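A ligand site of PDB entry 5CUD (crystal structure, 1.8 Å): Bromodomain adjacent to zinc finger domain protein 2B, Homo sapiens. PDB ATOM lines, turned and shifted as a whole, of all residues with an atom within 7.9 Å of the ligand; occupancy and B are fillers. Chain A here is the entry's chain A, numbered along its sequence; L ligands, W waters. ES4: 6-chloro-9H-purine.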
ATOM      1  N   TRP A  35     -15.912  25.941 -29.061  1.00  0.00           N
ATOM      2  CA  TRP A  35     -15.909  27.366 -28.706  1.00  0.00           C
ATOM      3  C   TRP A  35     -15.472  27.697 -27.257  1.00  0.00           C
ATOM      4  O   TRP A  35     -14.937  28.789 -27.037  1.00  0.00           O
ATOM      5  CB  TRP A  35     -17.294  27.987 -28.981  1.00  0.00           C
ATOM      6  CG  TRP A  35     -18.412  27.301 -28.291  1.00  0.00           C
ATOM      7  CD1 TRP A  35     -19.187  26.291 -28.783  1.00  0.00           C
ATOM      8  CD2 TRP A  35     -18.894  27.578 -26.973  1.00  0.00           C
ATOM      9  NE1 TRP A  35     -20.105  25.912 -27.846  1.00  0.00           N
ATOM     10  CE2 TRP A  35     -19.952  26.686 -26.718  1.00  0.00           C
ATOM     11  CE3 TRP A  35     -18.525  28.482 -25.967  1.00  0.00           C
ATOM     12  CZ2 TRP A  35     -20.649  26.674 -25.517  1.00  0.00           C
ATOM     13  CZ3 TRP A  35     -19.218  28.464 -24.784  1.00  0.00           C
ATOM     14  CH2 TRP A  35     -20.266  27.575 -24.561  1.00  0.00           C
ATOM     15  N   PRO A  36     -15.660  26.772 -26.287  1.00  0.00           N
ATOM     16  CA  PRO A  36     -15.138  27.179 -24.974  1.00  0.00           C
ATOM     17  C   PRO A  36     -13.621  27.125 -24.875  1.00  0.00           C
ATOM     18  O   PRO A  36     -13.090  27.582 -23.859  1.00  0.00           O
ATOM     19  CB  PRO A  36     -15.755  26.159 -24.001  1.00  0.00           C
ATOM     20  CG  PRO A  36     -16.889  25.521 -24.755  1.00  0.00           C
ATOM     21  CD  PRO A  36     -16.431  25.521 -26.185  1.00  0.00           C
ATOM     22  N   PHE A  37     -12.947  26.548 -25.878  1.00  0.00           N
ATOM     23  CA  PHE A  37     -11.549  26.129 -25.758  1.00  0.00           C
ATOM     24  C   PHE A  37     -10.617  26.796 -26.759  1.00  0.00           C
ATOM     25  O   PHE A  37      -9.404  26.553 -26.745  1.00  0.00           O
ATOM     26  CB  PHE A  37     -11.452  24.601 -25.910  1.00  0.00           C
ATOM     27  CG  PHE A  37     -12.468  23.866 -25.091  1.00  0.00           C
ATOM     28  CD1 PHE A  37     -12.445  23.938 -23.698  1.00  0.00           C
ATOM     29  CD2 PHE A  37     -13.469  23.112 -25.707  1.00  0.00           C
ATOM     30  CE1 PHE A  37     -13.407  23.286 -22.937  1.00  0.00           C
ATOM     31  CE2 PHE A  37     -14.429  22.439 -24.938  1.00  0.00           C
ATOM     32  CZ  PHE A  37     -14.393  22.527 -23.558  1.00  0.00           C
ATOM     33  N   LEU A  38     -11.175  27.634 -27.611  1.00  0.00           N
ATOM     34  CA  LEU A  38     -10.401  28.271 -28.673  1.00  0.00           C
ATOM     35  C   LEU A  38      -9.364  29.281 -28.159  1.00  0.00           C
ATOM     36  O   LEU A  38      -8.294  29.418 -28.747  1.00  0.00           O
ATOM     37  CB  LEU A  38     -11.332  28.950 -29.670  1.00  0.00           C
ATOM     38  CG  LEU A  38     -12.278  28.007 -30.424  1.00  0.00           C
ATOM     39  CD1 LEU A  38     -13.231  28.790 -31.289  1.00  0.00           C
ATOM     40  CD2 LEU A  38     -11.464  27.011 -31.259  1.00  0.00           C
ATOM     41  N   LEU A  39      -9.696  29.975 -27.079  1.00  0.00           N
ATOM     42  CA  LEU A  39      -8.845  31.013 -26.501  1.00  0.00           C
ATOM     43  C   LEU A  39      -8.644  30.810 -25.012  1.00  0.00           C
ATOM     44  O   LEU A  39      -9.446  30.137 -24.368  1.00  0.00           O
ATOM     45  CB  LEU A  39      -9.469  32.388 -26.773  1.00  0.00           C
ATOM     46  CG  LEU A  39      -9.551  32.828 -28.228  1.00  0.00           C
ATOM     47  CD1 LEU A  39     -10.306  34.161 -28.311  1.00  0.00           C
ATOM     48  CD2 LEU A  39      -8.157  32.962 -28.800  1.00  0.00           C
ATOM     49  N   PRO A  40      -7.578  31.394 -24.430  1.00  0.00           N
ATOM     50  CA  PRO A  40      -7.402  31.285 -22.980  1.00  0.00           C
ATOM     51  C   PRO A  40      -8.594  31.856 -22.243  1.00  0.00           C
ATOM     52  O   PRO A  40      -9.179  32.851 -22.700  1.00  0.00           O
ATOM     53  CB  PRO A  40      -6.145  32.113 -22.696  1.00  0.00           C
ATOM     54  CG  PRO A  40      -5.477  32.263 -23.996  1.00  0.00           C
ATOM     55  CD  PRO A  40      -6.532  32.241 -25.042  1.00  0.00           C
ATOM     56  N   VAL A  41      -8.988  31.205 -21.159  1.00  0.00           N
ATOM     57  CA  VAL A  41     -10.023  31.735 -20.272  1.00  0.00           C
ATOM     58  C   VAL A  41      -9.589  33.100 -19.768  1.00  0.00           C
ATOM     59  O   VAL A  41      -8.441  33.290 -19.377  1.00  0.00           O
ATOM     60  CB  VAL A  41     -10.282  30.784 -19.082  1.00  0.00           C
ATOM     61  CG1 VAL A  41     -11.219  31.453 -18.045  1.00  0.00           C
ATOM     62  CG2 VAL A  41     -10.849  29.459 -19.567  1.00  0.00           C
ATOM     63  N   ASN A  42     -10.506  34.060 -19.817  1.00  0.00           N
ATOM     64  CA  ASN A  42     -10.221  35.415 -19.347  1.00  0.00           C
ATOM     65  C   ASN A  42     -10.086  35.440 -17.833  1.00  0.00           C
ATOM     66  O   ASN A  42     -11.102  35.400 -17.124  1.00  0.00           O
ATOM     67  CB  ASN A  42     -11.317  36.385 -19.812  1.00  0.00           C
ATOM     68  CG  ASN A  42     -10.883  37.835 -19.729  1.00  0.00           C
ATOM     69  OD1 ASN A  42     -10.108  38.215 -18.844  1.00  0.00           O
ATOM     70  ND2 ASN A  42     -11.370  38.640 -20.661  1.00  0.00           N
ATOM     71  N   LEU A  45     -12.001  38.172 -15.971  1.00  0.00           N
ATOM     72  CA  LEU A  45     -13.459  38.227 -16.067  1.00  0.00           C
ATOM     73  C   LEU A  45     -14.129  36.956 -15.574  1.00  0.00           C
ATOM     74  O   LEU A  45     -15.354  36.870 -15.531  1.00  0.00           O
ATOM     75  CB  LEU A  45     -13.889  38.486 -17.512  1.00  0.00           C
ATOM     76  CG  LEU A  45     -13.363  39.763 -18.194  1.00  0.00           C
ATOM     77  CD1 LEU A  45     -14.117  40.017 -19.490  1.00  0.00           C
ATOM     78  CD2 LEU A  45     -13.463  40.981 -17.272  1.00  0.00           C
ATOM     79  N   VAL A  46     -13.345  35.953 -15.207  1.00  0.00           N
ATOM     80  CA  VAL A  46     -13.936  34.708 -14.736  1.00  0.00           C
ATOM     81  C   VAL A  46     -13.481  34.431 -13.311  1.00  0.00           C
ATOM     82  O   VAL A  46     -12.322  34.045 -13.076  1.00  0.00           O
ATOM     83  CB  VAL A  46     -13.580  33.519 -15.649  1.00  0.00           C
ATOM     84  CG1 VAL A  46     -14.147  32.218 -15.088  1.00  0.00           C
ATOM     85  CG2 VAL A  46     -14.106  33.759 -17.057  1.00  0.00           C
ATOM     86  N   PRO A  47     -14.395  34.648 -12.351  1.00  0.00           N
ATOM     87  CA  PRO A  47     -14.104  34.455 -10.930  1.00  0.00           C
ATOM     88  C   PRO A  47     -13.740  33.018 -10.603  1.00  0.00           C
ATOM     89  O   PRO A  47     -14.447  32.084 -11.007  1.00  0.00           O
ATOM     90  CB  PRO A  47     -15.427  34.864 -10.246  1.00  0.00           C
ATOM     91  CG  PRO A  47     -16.473  34.719 -11.290  1.00  0.00           C
ATOM     92  CD  PRO A  47     -15.786  35.059 -12.597  1.00  0.00           C
ATOM     93  N   TYR A  49     -11.177  31.205 -11.581  1.00  0.00           N
ATOM     94  CA  TYR A  49     -10.378  30.417 -12.524  1.00  0.00           C
ATOM     95  C   TYR A  49      -8.886  30.451 -12.244  1.00  0.00           C
ATOM     96  O   TYR A  49      -8.216  29.413 -12.262  1.00  0.00           O
ATOM     97  CB  TYR A  49     -10.635  30.849 -13.976  1.00  0.00           C
ATOM     98  CG  TYR A  49     -10.420  29.693 -14.924  1.00  0.00           C
ATOM     99  CD1 TYR A  49     -11.453  28.814 -15.210  1.00  0.00           C
ATOM    100  CD2 TYR A  49      -9.187  29.453 -15.493  1.00  0.00           C
ATOM    101  CE1 TYR A  49     -11.263  27.730 -16.059  1.00  0.00           C
ATOM    102  CE2 TYR A  49      -8.972  28.387 -16.364  1.00  0.00           C
ATOM    103  CZ  TYR A  49     -10.014  27.522 -16.636  1.00  0.00           C
ATOM    104  OH  TYR A  49      -9.816  26.444 -17.485  1.00  0.00           O
ATOM    105  N   ILE A  53      -7.494  26.683 -11.214  1.00  0.00           N
ATOM    106  CA  ILE A  53      -6.868  25.983 -12.349  1.00  0.00           C
ATOM    107  C   ILE A  53      -5.394  26.346 -12.470  1.00  0.00           C
ATOM    108  O   ILE A  53      -5.046  27.398 -13.010  1.00  0.00           O
ATOM    109  CB  ILE A  53      -7.593  26.286 -13.687  1.00  0.00           C
ATOM    110  CG1 ILE A  53      -9.073  25.949 -13.609  1.00  0.00           C
ATOM    111  CG2 ILE A  53      -6.916  25.525 -14.854  1.00  0.00           C
ATOM    112  CD1 ILE A  53      -9.374  24.454 -13.415  1.00  0.00           C
ATOM    113  N   MET A  57      -4.913  25.888 -20.126  1.00  0.00           N
ATOM    114  CA  MET A  57      -4.503  25.501 -21.466  1.00  0.00           C
ATOM    115  C   MET A  57      -5.705  25.663 -22.395  1.00  0.00           C
ATOM    116  O   MET A  57      -6.873  25.554 -21.960  1.00  0.00           O
ATOM    117  CB  MET A  57      -3.954  24.067 -21.497  1.00  0.00           C
ATOM    118  CG  MET A  57      -3.353  23.646 -22.843  1.00  0.00           C
ATOM    119  SD  MET A  57      -2.084  24.774 -23.465  1.00  0.00           S
ATOM    120  CE  MET A  57      -0.894  24.783 -22.132  1.00  0.00           C
ATOM    121  N   VAL A  84      -6.612  20.533 -21.394  1.00  0.00           N
ATOM    122  CA  VAL A  84      -7.760  21.378 -21.709  1.00  0.00           C
ATOM    123  C   VAL A  84      -9.056  20.767 -21.154  1.00  0.00           C
ATOM    124  O   VAL A  84      -9.866  21.453 -20.527  1.00  0.00           O
ATOM    125  CB  VAL A  84      -7.924  21.598 -23.239  1.00  0.00           C
ATOM    126  CG1 VAL A  84      -9.201  22.365 -23.515  1.00  0.00           C
ATOM    127  CG2 VAL A  84      -6.707  22.367 -23.814  1.00  0.00           C
ATOM    128  N   ASN A  87      -9.049  20.407 -17.170  1.00  0.00           N
ATOM    129  CA  ASN A  87      -9.391  21.711 -16.587  1.00  0.00           C
ATOM    130  C   ASN A  87     -10.887  22.005 -16.699  1.00  0.00           C
ATOM    131  O   ASN A  87     -11.491  22.552 -15.766  1.00  0.00           O
ATOM    132  CB  ASN A  87      -8.625  22.841 -17.279  1.00  0.00           C
ATOM    133  CG  ASN A  87      -7.140  22.848 -16.915  1.00  0.00           C
ATOM    134  OD1 ASN A  87      -6.723  22.240 -15.939  1.00  0.00           O
ATOM    135  ND2 ASN A  87      -6.346  23.574 -17.699  1.00  0.00           N
ATOM    136  N   CYS A  88     -11.466  21.644 -17.847  1.00  0.00           N
ATOM    137  CA  CYS A  88     -12.888  21.884 -18.085  1.00  0.00           C
ATOM    138  C   CYS A  88     -13.739  21.111 -17.092  1.00  0.00           C
ATOM    139  O   CYS A  88     -14.712  21.648 -16.551  1.00  0.00           O
ATOM    140  CB  CYS A  88     -13.276  21.515 -19.520  1.00  0.00           C
ATOM    141  SG  CYS A  88     -15.026  21.768 -19.952  1.00  0.00           S
ATOM    142  N   GLU A  89     -13.372  19.854 -16.848  1.00  0.00           N
ATOM    143  CA  GLU A  89     -14.093  19.012 -15.876  1.00  0.00           C
ATOM    144  C   GLU A  89     -13.968  19.508 -14.441  1.00  0.00           C
ATOM    145  O   GLU A  89     -14.914  19.396 -13.658  1.00  0.00           O
ATOM    146  CB  GLU A  89     -13.594  17.562 -15.924  1.00  0.00           C
ATOM    147  CG  GLU A  89     -14.214  16.752 -17.013  1.00  0.00           C
ATOM    148  CD  GLU A  89     -14.114  15.264 -16.755  1.00  0.00           C
ATOM    149  OE1 GLU A  89     -14.516  14.806 -15.663  1.00  0.00           O
ATOM    150  OE2 GLU A  89     -13.642  14.553 -17.664  1.00  0.00           O
ATOM    151  N   PHE A  91     -13.731  22.580 -13.459  1.00  0.00           N
ATOM    152  CA  PHE A  91     -14.377  23.866 -13.238  1.00  0.00           C
ATOM    153  C   PHE A  91     -15.859  23.911 -13.630  1.00  0.00           C
ATOM    154  O   PHE A  91     -16.602  24.829 -13.219  1.00  0.00           O
ATOM    155  CB  PHE A  91     -13.618  24.954 -14.004  1.00  0.00           C
ATOM    156  CG  PHE A  91     -13.816  26.333 -13.455  1.00  0.00           C
ATOM    157  CD1 PHE A  91     -13.119  26.753 -12.342  1.00  0.00           C
ATOM    158  CD2 PHE A  91     -14.688  27.221 -14.065  1.00  0.00           C
ATOM    159  CE1 PHE A  91     -13.279  28.037 -11.827  1.00  0.00           C
ATOM    160  CE2 PHE A  91     -14.858  28.504 -13.563  1.00  0.00           C
ATOM    161  CZ  PHE A  91     -14.156  28.916 -12.446  1.00  0.00           C
ATOM    162  N   ASN A  92     -16.311  22.965 -14.435  1.00  0.00           N
ATOM    163  CA  ASN A  92     -17.701  22.980 -14.903  1.00  0.00           C
ATOM    164  C   ASN A  92     -18.465  21.710 -14.542  1.00  0.00           C
ATOM    165  O   ASN A  92     -17.898  20.610 -14.499  1.00  0.00           O
ATOM    166  CB  ASN A  92     -17.778  23.213 -16.415  1.00  0.00           C
ATOM    167  CG  ASN A  92     -16.988  24.427 -16.869  1.00  0.00           C
ATOM    168  OD1 ASN A  92     -15.770  24.364 -17.069  1.00  0.00           O
ATOM    169  ND2 ASN A  92     -17.684  25.527 -17.053  1.00  0.00           N
ATOM    170  N   ILE A  98     -20.826  24.021 -21.326  1.00  0.00           N
ATOM    171  CA  ILE A  98     -19.369  23.918 -21.399  1.00  0.00           C
ATOM    172  C   ILE A  98     -18.900  22.537 -20.967  1.00  0.00           C
ATOM    173  O   ILE A  98     -18.010  21.946 -21.586  1.00  0.00           O
ATOM    174  CB  ILE A  98     -18.677  25.008 -20.541  1.00  0.00           C
ATOM    175  CG1 ILE A  98     -18.978  26.393 -21.128  1.00  0.00           C
ATOM    176  CG2 ILE A  98     -17.173  24.756 -20.430  1.00  0.00           C
ATOM    177  CD1 ILE A  98     -18.553  27.522 -20.208  1.00  0.00           C
ATOM    178  N   GLY A  99     -19.529  22.008 -19.928  1.00  0.00           N
ATOM    179  CA  GLY A  99     -19.193  20.698 -19.391  1.00  0.00           C
ATOM    180  C   GLY A  99     -19.456  19.597 -20.411  1.00  0.00           C
ATOM    181  O   GLY A  99     -18.622  18.718 -20.607  1.00  0.00           O
HETATM  182  C10 ES4 L   1     -14.628  28.590 -19.926  1.00  0.00           C
HETATM  183 CL01 ES4 L   1     -14.702  30.506 -21.901  1.00  0.00          CL
HETATM  184  C02 ES4 L   1     -15.082  29.891 -20.304  1.00  0.00           C
HETATM  185  N03 ES4 L   1     -15.772  30.625 -19.403  1.00  0.00           N
HETATM  186  C04 ES4 L   1     -16.057  30.131 -18.172  1.00  0.00           C
HETATM  187  N05 ES4 L   1     -15.638  28.901 -17.815  1.00  0.00           N
HETATM  188  C06 ES4 L   1     -14.918  28.103 -18.676  1.00  0.00           C
HETATM  189  N07 ES4 L   1     -14.373  26.835 -18.603  1.00  0.00           N
HETATM  190  C08 ES4 L   1     -13.767  26.566 -19.783  1.00  0.00           C
HETATM  191  N09 ES4 L   1     -13.919  27.621 -20.599  1.00  0.00           N
HETATM  192  O   HOH W   1     -16.187  30.854 -23.866  1.00  0.00           O
HETATM  193  O   HOH W   2     -12.268  31.702 -23.856  1.00  0.00           O
HETATM  194  O   HOH W   3     -11.875  25.087 -18.424  1.00  0.00           O
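The side-chain amide oxygen of Asn 92 lies close to the backbone carbonyl oxygen of Cys 88, at 3.0 Å. The backbone carbonyl oxygen of Ile 98 is in hydrogen-bond range of the side-chain sulfur of Cys 88, at 3.4 Å.
A nitrogen (N07) of the ligand is in hydrogen-bond range of the side-chain amide oxygen (OD1) of Asn 92, 3.2 Å away. O of Pro 36 sits close to N09 of the ligand (3.4 Å).
Val 41 touches the ligand (CG2 to N09, 3.7 Å). Ile 98 touches the ligand (CG2 to C08, 3.9 Å). Hydrophobic or aromatic side chains that line the ligand: Val 41 and Ile 98. The nearest printed residue that does not touch the ligand is Tyr 49 (4.1 Å).
Water W3 lies within hydrogen-bond range of OH of Tyr 49 (2.6 Å) and N07 of the ligand (3.1 Å).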
